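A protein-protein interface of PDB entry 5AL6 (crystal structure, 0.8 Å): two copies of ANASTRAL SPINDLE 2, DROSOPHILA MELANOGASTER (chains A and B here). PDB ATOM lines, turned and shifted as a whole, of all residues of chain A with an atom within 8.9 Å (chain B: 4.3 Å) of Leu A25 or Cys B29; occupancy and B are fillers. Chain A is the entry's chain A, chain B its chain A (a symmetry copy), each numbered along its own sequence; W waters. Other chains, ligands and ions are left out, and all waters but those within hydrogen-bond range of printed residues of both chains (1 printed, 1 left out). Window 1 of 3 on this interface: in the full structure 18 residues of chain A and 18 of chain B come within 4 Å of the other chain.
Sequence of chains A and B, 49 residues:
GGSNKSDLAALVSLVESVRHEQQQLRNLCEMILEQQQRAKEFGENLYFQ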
ATOM      1  N   VAL A  18      10.242 -20.164  14.144  1.00  0.00           N
ATOM      2  CA  VAL A  18       9.586 -20.728  15.329  1.00  0.00           C
ATOM      3  C   VAL A  18       9.082 -19.598  16.246  1.00  0.00           C
ATOM      4  O   VAL A  18       7.960 -19.655  16.772  1.00  0.00           O
ATOM      5  CB  VAL A  18      10.551 -21.677  16.081  1.00  0.00           C
ATOM      6  CG1 VAL A  18       9.989 -22.092  17.449  1.00  0.00           C
ATOM      7  CG2 VAL A  18      10.843 -22.907  15.232  1.00  0.00           C
ATOM      8  N   ARG A  19       9.925 -18.576  16.454  1.00  0.00           N
ATOM      9  CA  ARG A  19       9.548 -17.475  17.336  1.00  0.00           C
ATOM     10  C   ARG A  19       8.313 -16.720  16.808  1.00  0.00           C
ATOM     11  O   ARG A  19       7.402 -16.375  17.573  1.00  0.00           O
ATOM     12  CB  ARG A  19      10.748 -16.519  17.488  1.00  0.00           C
ATOM     13  CG  ARG A  19      10.530 -15.502  18.608  1.00  0.00           C
ATOM     14  CD  ARG A  19      11.629 -14.446  18.612  1.00  0.00           C
ATOM     15  NE  ARG A  19      11.430 -13.537  19.729  1.00  0.00           N
ATOM     16  CZ  ARG A  19      12.116 -12.399  19.859  1.00  0.00           C
ATOM     17  NH1 ARG A  19      13.007 -12.016  18.948  1.00  0.00           N
ATOM     18  NH2 ARG A  19      11.901 -11.649  20.940  1.00  0.00           N
ATOM     19  N   HIS A  20       8.307 -16.446  15.491  1.00  0.00           N
ATOM     20  CA  HIS A  20       7.182 -15.773  14.843  1.00  0.00           C
ATOM     21  C   HIS A  20       5.900 -16.608  14.971  1.00  0.00           C
ATOM     22  O   HIS A  20       4.841 -16.086  15.353  1.00  0.00           O
ATOM     23  CB  HIS A  20       7.540 -15.556  13.356  1.00  0.00           C
ATOM     24  CG  HIS A  20       6.350 -15.291  12.453  1.00  0.00           C
ATOM     25  ND1 HIS A  20       5.578 -14.169  12.577  1.00  0.00           N
ATOM     26  CD2 HIS A  20       5.830 -16.039  11.453  1.00  0.00           C
ATOM     27  CE1 HIS A  20       4.646 -14.207  11.650  1.00  0.00           C
ATOM     28  NE2 HIS A  20       4.766 -15.347  10.966  1.00  0.00           N
ATOM     29  N   GLU A  21       5.987 -17.895  14.653  1.00  0.00           N
ATOM     30  CA  GLU A  21       4.820 -18.768  14.747  1.00  0.00           C
ATOM     31  C   GLU A  21       4.316 -18.852  16.189  1.00  0.00           C
ATOM     32  O   GLU A  21       3.107 -18.956  16.434  1.00  0.00           O
ATOM     33  CB  GLU A  21       5.153 -20.135  14.136  1.00  0.00           C
ATOM     34  CG  GLU A  21       5.279 -19.992  12.615  1.00  0.00           C
ATOM     35  CD  GLU A  21       6.087 -21.042  11.879  1.00  0.00           C
ATOM     36  OE1 GLU A  21       6.482 -22.078  12.448  1.00  0.00           O
ATOM     37  OE2 GLU A  21       6.385 -20.735  10.668  1.00  0.00           O
ATOM     38  N   GLN A  22       5.233 -18.777  17.159  1.00  0.00           N
ATOM     39  CA  GLN A  22       4.816 -18.793  18.561  1.00  0.00           C
ATOM     40  C   GLN A  22       4.028 -17.528  18.907  1.00  0.00           C
ATOM     41  O   GLN A  22       3.059 -17.595  19.673  1.00  0.00           O
ATOM     42  CB  GLN A  22       6.033 -18.976  19.469  1.00  0.00           C
ATOM     43  CG  GLN A  22       5.616 -19.141  20.931  1.00  0.00           C
ATOM     44  CD  GLN A  22       6.789 -19.608  21.757  1.00  0.00           C
ATOM     45  OE1 GLN A  22       6.892 -20.787  22.139  1.00  0.00           O
ATOM     46  NE2 GLN A  22       7.724 -18.691  22.031  1.00  0.00           N
ATOM     47  N   GLN A  23       4.437 -16.369  18.364  1.00  0.00           N
ATOM     48  CA  GLN A  23       3.669 -15.147  18.602  1.00  0.00           C
ATOM     49  C   GLN A  23       2.292 -15.205  17.931  1.00  0.00           C
ATOM     50  O   GLN A  23       1.318 -14.682  18.503  1.00  0.00           O
ATOM     51  CB  GLN A  23       4.460 -13.912  18.141  1.00  0.00           C
ATOM     52  CG  GLN A  23       3.752 -12.595  18.469  1.00  0.00           C
ATOM     53  CD  GLN A  23       3.667 -12.330  19.953  1.00  0.00           C
ATOM     54  OE1 GLN A  23       4.625 -12.567  20.698  1.00  0.00           O
ATOM     55  NE2 GLN A  23       2.534 -11.812  20.395  1.00  0.00           N
ATOM     56  N   GLN A  24       2.198 -15.811  16.754  1.00  0.00           N
ATOM     57  CA  GLN A  24       0.875 -15.988  16.159  1.00  0.00           C
ATOM     58  C   GLN A  24      -0.023 -16.823  17.103  1.00  0.00           C
ATOM     59  O   GLN A  24      -1.214 -16.534  17.293  1.00  0.00           O
ATOM     60  CB  GLN A  24       0.974 -16.695  14.799  1.00  0.00           C
ATOM     61  CG  GLN A  24       1.675 -15.885  13.723  1.00  0.00           C
ATOM     62  CD  GLN A  24       1.670 -16.695  12.408  1.00  0.00           C
ATOM     63  OE1 GLN A  24       1.815 -17.973  12.379  1.00  0.00           O
ATOM     64  NE2 GLN A  24       1.457 -16.007  11.289  1.00  0.00           N
ATOM     65  N   LEU A  25       0.567 -17.864  17.692  1.00  0.00           N
ATOM     66  CA  LEU A  25      -0.152 -18.695  18.657  1.00  0.00           C
ATOM     67  C   LEU A  25      -0.527 -17.888  19.914  1.00  0.00           C
ATOM     68  O   LEU A  25      -1.644 -18.018  20.421  1.00  0.00           O
ATOM     69  CB  LEU A  25       0.726 -19.920  18.981  1.00  0.00           C
ATOM     70  CG  LEU A  25       0.161 -20.853  20.045  1.00  0.00           C
ATOM     71  CD1 LEU A  25      -1.232 -21.374  19.690  1.00  0.00           C
ATOM     72  CD2 LEU A  25       1.144 -21.993  20.270  1.00  0.00           C
ATOM     73  N   ARG A  26       0.398 -17.059  20.415  1.00  0.00           N
ATOM     74  CA  ARG A  26       0.092 -16.186  21.541  1.00  0.00           C
ATOM     75  C   ARG A  26      -1.101 -15.276  21.225  1.00  0.00           C
ATOM     76  O   ARG A  26      -2.001 -15.124  22.066  1.00  0.00           O
ATOM     77  CB  ARG A  26       1.351 -15.360  21.876  1.00  0.00           C
ATOM     78  CG  ARG A  26       1.155 -14.231  22.861  1.00  0.00           C
ATOM     79  CD  ARG A  26       0.793 -14.729  24.262  1.00  0.00           C
ATOM     80  NE  ARG A  26       0.642 -13.624  25.204  1.00  0.00           N
ATOM     81  CZ  ARG A  26       1.636 -12.988  25.761  1.00  0.00           C
ATOM     82  NH1 ARG A  26       2.879 -13.399  25.614  1.00  0.00           N
ATOM     83  NH2 ARG A  26       1.366 -11.953  26.544  1.00  0.00           N
ATOM     84  N   ASN A  27      -1.098 -14.668  20.034  1.00  0.00           N
ATOM     85  CA  ASN A  27      -2.193 -13.769  19.691  1.00  0.00           C
ATOM     86  C   ASN A  27      -3.527 -14.535  19.621  1.00  0.00           C
ATOM     87  O   ASN A  27      -4.564 -14.018  20.063  1.00  0.00           O
ATOM     88  CB  ASN A  27      -1.854 -13.067  18.372  1.00  0.00           C
ATOM     89  CG  ASN A  27      -0.708 -12.040  18.546  1.00  0.00           C
ATOM     90  OD1 ASN A  27      -0.356 -11.657  19.650  1.00  0.00           O
ATOM     91  ND2 ASN A  27      -0.095 -11.653  17.439  1.00  0.00           N
ATOM     92  N   LEU A  28      -3.501 -15.760  19.098  1.00  0.00           N
ATOM     93  CA  LEU A  28      -4.691 -16.605  19.085  1.00  0.00           C
ATOM     94  C   LEU A  28      -5.170 -16.886  20.517  1.00  0.00           C
ATOM     95  O   LEU A  28      -6.369 -16.805  20.811  1.00  0.00           O
ATOM     96  CB  LEU A  28      -4.361 -17.915  18.342  1.00  0.00           C
ATOM     97  CG  LEU A  28      -5.405 -19.018  18.477  1.00  0.00           C
ATOM     98  CD1 LEU A  28      -6.772 -18.644  17.937  1.00  0.00           C
ATOM     99  CD2 LEU A  28      -4.897 -20.267  17.769  1.00  0.00           C
ATOM    100  N   CYS A  29      -4.244 -17.235  21.411  1.00  0.00           N
ATOM    101  CA  CYS A  29      -4.637 -17.548  22.781  1.00  0.00           C
ATOM    102  C   CYS A  29      -5.174 -16.297  23.517  1.00  0.00           C
ATOM    103  O   CYS A  29      -6.066 -16.438  24.358  1.00  0.00           O
ATOM    104  CB  CYS A  29      -3.508 -18.245  23.528  1.00  0.00           C
ATOM    105  SG  CYS A  29      -3.221 -19.944  22.941  1.00  0.00           S
ATOM    106  N   GLU A  30      -4.654 -15.110  23.199  1.00  0.00           N
ATOM    107  CA  GLU A  30      -5.246 -13.905  23.764  1.00  0.00           C
ATOM    108  C   GLU A  30      -6.714 -13.752  23.286  1.00  0.00           C
ATOM    109  O   GLU A  30      -7.586 -13.366  24.077  1.00  0.00           O
ATOM    110  CB  GLU A  30      -4.451 -12.654  23.380  1.00  0.00           C
ATOM    111  CG  GLU A  30      -3.015 -12.615  23.921  1.00  0.00           C
ATOM    112  CD  GLU A  30      -2.900 -12.248  25.380  1.00  0.00           C
ATOM    113  OE1 GLU A  30      -3.911 -11.981  26.050  1.00  0.00           O
ATOM    114  OE2 GLU A  30      -1.761 -12.289  25.901  1.00  0.00           O
ATOM    115  N   MET A  31      -6.973 -14.054  22.018  1.00  0.00           N
ATOM    116  CA  MET A  31      -8.344 -14.022  21.513  1.00  0.00           C
ATOM    117  C   MET A  31      -9.220 -15.058  22.226  1.00  0.00           C
ATOM    118  O   MET A  31     -10.401 -14.784  22.512  1.00  0.00           O
ATOM    119  CB  MET A  31      -8.380 -14.245  19.984  1.00  0.00           C
ATOM    120  CG  MET A  31      -7.625 -13.194  19.183  1.00  0.00           C
ATOM    121  SD  MET A  31      -8.291 -11.530  19.358  1.00  0.00           S
ATOM    122  CE  MET A  31      -9.616 -11.617  18.156  1.00  0.00           C
ATOM    123  N   ILE A  32      -8.681 -16.247  22.496  1.00  0.00           N
ATOM    124  CA  ILE A  32      -9.434 -17.253  23.250  1.00  0.00           C
ATOM    125  C   ILE A  32      -9.823 -16.705  24.631  1.00  0.00           C
ATOM    126  O   ILE A  32     -10.979 -16.826  25.053  1.00  0.00           O
ATOM    127  CB  ILE A  32      -8.622 -18.566  23.378  1.00  0.00           C
ATOM    128  CG1 ILE A  32      -8.497 -19.263  22.017  1.00  0.00           C
ATOM    129  CG2 ILE A  32      -9.244 -19.508  24.416  1.00  0.00           C
ATOM    130  CD1 ILE A  32      -7.500 -20.408  21.971  1.00  0.00           C
ATOM    131  N   GLN A  35     -12.553 -13.879  24.276  1.00  0.00           N
ATOM    132  CA  GLN A  35     -13.862 -14.399  23.907  1.00  0.00           C
ATOM    133  C   GLN A  35     -14.500 -15.169  25.068  1.00  0.00           C
ATOM    134  O   GLN A  35     -15.700 -15.008  25.334  1.00  0.00           O
ATOM    135  CB  GLN A  35     -13.747 -15.261  22.643  1.00  0.00           C
ATOM    136  CG  GLN A  35     -15.094 -15.932  22.226  1.00  0.00           C
ATOM    137  CD  GLN A  35     -14.887 -16.946  21.031  1.00  0.00           C
ATOM    138  OE1 GLN A  35     -14.205 -18.013  21.218  1.00  0.00           O
ATOM    139  NE2 GLN A  35     -15.375 -16.650  19.887  1.00  0.00           N
ATOM    140  N   LEU B  25       0.113 -27.852  18.188  1.00  0.00           N
ATOM    141  CA  LEU B  25      -0.478 -27.064  19.268  1.00  0.00           C
ATOM    142  C   LEU B  25      -1.334 -25.912  18.710  1.00  0.00           C
ATOM    143  O   LEU B  25      -2.428 -25.652  19.218  1.00  0.00           O
ATOM    144  CB  LEU B  25       0.664 -26.565  20.177  1.00  0.00           C
ATOM    145  CG  LEU B  25       0.228 -25.648  21.313  1.00  0.00           C
ATOM    146  CD1 LEU B  25      -0.824 -26.291  22.217  1.00  0.00           C
ATOM    147  CD2 LEU B  25       1.459 -25.224  22.101  1.00  0.00           C
ATOM    148  N   ARG B  26      -0.844 -25.224  17.671  1.00  0.00           N
ATOM    149  CA  ARG B  26      -1.632 -24.185  17.020  1.00  0.00           C
ATOM    150  C   ARG B  26      -2.965 -24.743  16.508  1.00  0.00           C
ATOM    151  O   ARG B  26      -4.015 -24.111  16.706  1.00  0.00           O
ATOM    152  CB  ARG B  26      -0.797 -23.589  15.867  1.00  0.00           C
ATOM    153  CG  ARG B  26      -1.537 -22.664  14.929  1.00  0.00           C
ATOM    154  CD  ARG B  26      -1.992 -21.373  15.612  1.00  0.00           C
ATOM    155  NE  ARG B  26      -2.674 -20.481  14.680  1.00  0.00           N
ATOM    156  CZ  ARG B  26      -2.068 -19.724  13.806  1.00  0.00           C
ATOM    157  NH1 ARG B  26      -0.756 -19.606  13.796  1.00  0.00           N
ATOM    158  NH2 ARG B  26      -2.806 -19.013  12.966  1.00  0.00           N
ATOM    159  N   ASN B  27      -2.920 -25.904  15.847  1.00  0.00           N
ATOM    160  CA  ASN B  27      -4.154 -26.468  15.315  1.00  0.00           C
ATOM    161  C   ASN B  27      -5.129 -26.821  16.453  1.00  0.00           C
ATOM    162  O   ASN B  27      -6.344 -26.606  16.319  1.00  0.00           O
ATOM    163  CB  ASN B  27      -3.802 -27.684  14.450  1.00  0.00           C
ATOM    164  CG  ASN B  27      -3.106 -27.269  13.130  1.00  0.00           C
ATOM    165  OD1 ASN B  27      -3.122 -26.113  12.736  1.00  0.00           O
ATOM    166  ND2 ASN B  27      -2.442 -28.219  12.494  1.00  0.00           N
ATOM    167  N   LEU B  28      -4.608 -27.331  17.567  1.00  0.00           N
ATOM    168  CA  LEU B  28      -5.437 -27.598  18.739  1.00  0.00           C
ATOM    169  C   LEU B  28      -6.075 -26.300  19.257  1.00  0.00           C
ATOM    170  O   LEU B  28      -7.270 -26.266  19.576  1.00  0.00           O
ATOM    171  CB  LEU B  28      -4.563 -28.258  19.824  1.00  0.00           C
ATOM    172  CG  LEU B  28      -5.203 -28.351  21.205  1.00  0.00           C
ATOM    173  CD1 LEU B  28      -6.481 -29.166  21.240  1.00  0.00           C
ATOM    174  CD2 LEU B  28      -4.190 -28.940  22.178  1.00  0.00           C
ATOM    175  N   CYS B  29      -5.284 -25.232  19.361  1.00  0.00           N
ATOM    176  CA  CYS B  29      -5.821 -23.977  19.877  1.00  0.00           C
ATOM    177  C   CYS B  29      -6.865 -23.367  18.912  1.00  0.00           C
ATOM    178  O   CYS B  29      -7.814 -22.734  19.385  1.00  0.00           O
ATOM    179  CB  CYS B  29      -4.699 -23.011  20.237  1.00  0.00           C
ATOM    180  SG  CYS B  29      -3.772 -23.529  21.715  1.00  0.00           S
ATOM    181  N   GLU B  30      -6.701 -23.564  17.603  1.00  0.00           N
ATOM    182  CA  GLU B  30      -7.749 -23.133  16.687  1.00  0.00           C
ATOM    183  C   GLU B  30      -9.062 -23.910  16.968  1.00  0.00           C
ATOM    184  O   GLU B  30     -10.151 -23.320  16.931  1.00  0.00           O
ATOM    185  CB  GLU B  30      -7.337 -23.337  15.226  1.00  0.00           C
ATOM    186  CG  GLU B  30      -6.128 -22.505  14.778  1.00  0.00           C
ATOM    187  CD  GLU B  30      -6.430 -21.053  14.498  1.00  0.00           C
ATOM    188  OE1 GLU B  30      -7.585 -20.611  14.609  1.00  0.00           O
ATOM    189  OE2 GLU B  30      -5.466 -20.303  14.217  1.00  0.00           O
ATOM    190  N   MET B  31      -8.952 -25.205  17.245  1.00  0.00           N
ATOM    191  CA  MET B  31     -10.131 -25.988  17.608  1.00  0.00           C
ATOM    192  C   MET B  31     -10.752 -25.480  18.914  1.00  0.00           C
ATOM    193  O   MET B  31     -11.991 -25.449  19.045  1.00  0.00           O
ATOM    194  CB  MET B  31      -9.789 -27.491  17.722  1.00  0.00           C
ATOM    195  CG  MET B  31      -9.267 -28.111  16.434  1.00  0.00           C
ATOM    196  SD  MET B  31     -10.452 -28.076  15.079  1.00  0.00           S
ATOM    197  CE  MET B  31     -11.413 -29.530  15.491  1.00  0.00           C
ATOM    198  N   ILE B  32      -9.925 -25.106  19.890  1.00  0.00           N
ATOM    199  CA  ILE B  32     -10.450 -24.531  21.132  1.00  0.00           C
ATOM    200  C   ILE B  32     -11.261 -23.262  20.833  1.00  0.00           C
ATOM    201  O   ILE B  32     -12.377 -23.095  21.339  1.00  0.00           O
ATOM    202  CB  ILE B  32      -9.302 -24.239  22.131  1.00  0.00           C
ATOM    203  CG1 ILE B  32      -8.692 -25.546  22.656  1.00  0.00           C
ATOM    204  CG2 ILE B  32      -9.782 -23.359  23.291  1.00  0.00           C
ATOM    205  CD1 ILE B  32      -7.392 -25.384  23.425  1.00  0.00           C
ATOM    206  N   LEU B  33     -10.692 -22.362  20.027  1.00  0.00           N
ATOM    207  CA  LEU B  33     -11.390 -21.117  19.700  1.00  0.00           C
ATOM    208  C   LEU B  33     -12.733 -21.417  19.018  1.00  0.00           C
ATOM    209  O   LEU B  33     -13.765 -20.821  19.353  1.00  0.00           O
ATOM    210  CB  LEU B  33     -10.517 -20.242  18.805  1.00  0.00           C
ATOM    211  CG  LEU B  33     -11.129 -18.889  18.430  1.00  0.00           C
ATOM    212  CD1 LEU B  33     -11.068 -17.898  19.598  1.00  0.00           C
ATOM    213  CD2 LEU B  33     -10.410 -18.278  17.213  1.00  0.00           C
HETATM  214  O   HOH W   1       1.341 -20.855  15.329  1.00  0.00           O
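The backbone carbonyl oxygen (O) of Leu B33 lies close to the side-chain amide oxygen (OE1) of Gln A35, 3.4 Å away. The guanidinium group (NH1) of Arg B26 is in hydrogen-bond range of the side-chain amide oxygen (OE1) of Gln A24 (3.4 Å).
OE2 of Glu B30 lies within salt-bridge range of NE of Arg B26. The side-chain amide nitrogen of Gln A24 sits at hydrogen-bond distance from a ring nitrogen (NE2) of His A20 (3.4 Å). SG of Cys A29 lies within hydrogen-bond range of O of Leu A25. The backbone carbonyl oxygen (O) of Leu B25 lies within hydrogen-bond range of the side-chain sulfur (SG) of Cys B29 (3.5 Å).
Leu A25 touches Leu B25 (CD2 to CD2, 3.7 Å). CA of Arg B26 touches CD1 of Leu A25 (3.9 Å). Cys B29 touches Leu A25. CD2 of Leu A28 touches CD of Arg B26, 3.8 Å away. Leu A28 touches Cys B29. Leu A28 touches Glu B30. Leu A28 touches Leu B33. Ile A32 touches Cys B29. Ile A32 touches Ile B32 (CD1 to CG2, 3.96 Å). CD1 of Leu B33 touches CG1 of Ile A32, at 3.8 Å.
Leu A25 touches just these residues of chain B: Leu B25, Arg B26 and Cys B29. Cys B29 touches just these residues of chain A: Leu A25 (3.9 Å), Leu A28 (3.7 Å), Cys A29 (3.8 Å) and Ile A32 (3.5 Å). No residue of chain A comes within 4 Å of Leu B28. Printed residues of chain A within 4 Å of Arg B26: Gln A24, Leu A25 and Leu A28. Of the printed residues of chain B, Leu A28 touches Arg B26, Cys B29, Glu B30 and Leu B33. Printed residues of chain B within 4 Å of Ile A32: Cys B29 (3.5 Å), Ile B32 (3.96 Å) and Leu B33 (3.8 Å). Of the printed residues of chain A, Leu B33 touches Leu A28 (3.7 Å), Ile A32 (3.8 Å) and Gln A35 (3.4 Å). Printed residues of chain A within 4 Å of Ile B32: Ile A32 (3.96 Å). Arg A19 touches none of the printed residues of chain B. Gln A22 touches none of the printed residues of chain B.
Of the 16 printed residues of chain A, 6 touch a printed residue of chain B. Hydrophobic or aromatic side chains of chain A within 4 Å of the printed part of chain B: Leu A25, Leu A28 and Ile A32. Hydrophobic or aromatic side chains of chain B within 4 Å of the printed part of chain A: Leu B25, Ile B32 and Leu B33. Among the printed residues, no Asp or Glu carboxylate lies within 4 Å of a Lys or Arg side-chain nitrogen of the other chain.
Leu A25 touches Cys B29, but with the chains exchanged Cys A29 does not touch Leu B25 (6.8 Å). Leu A28 touches Arg B26, but with the chains exchanged Arg A26 does not touch Leu B28 (11.3 Å). Ile A32 touches Cys B29, but with the chains exchanged Cys A29 does not touch Ile B32 (6.9 Å). Ile A32 touches its own counterpart, Ile B32. Positions printed for both chains: 25, 26, 27, 28, 29, 30, 31 and 32.
Water W1 lies within hydrogen-bond range of O of Glu A21 (2.8 Å) and NH1 of Arg B26 (2.9 Å).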
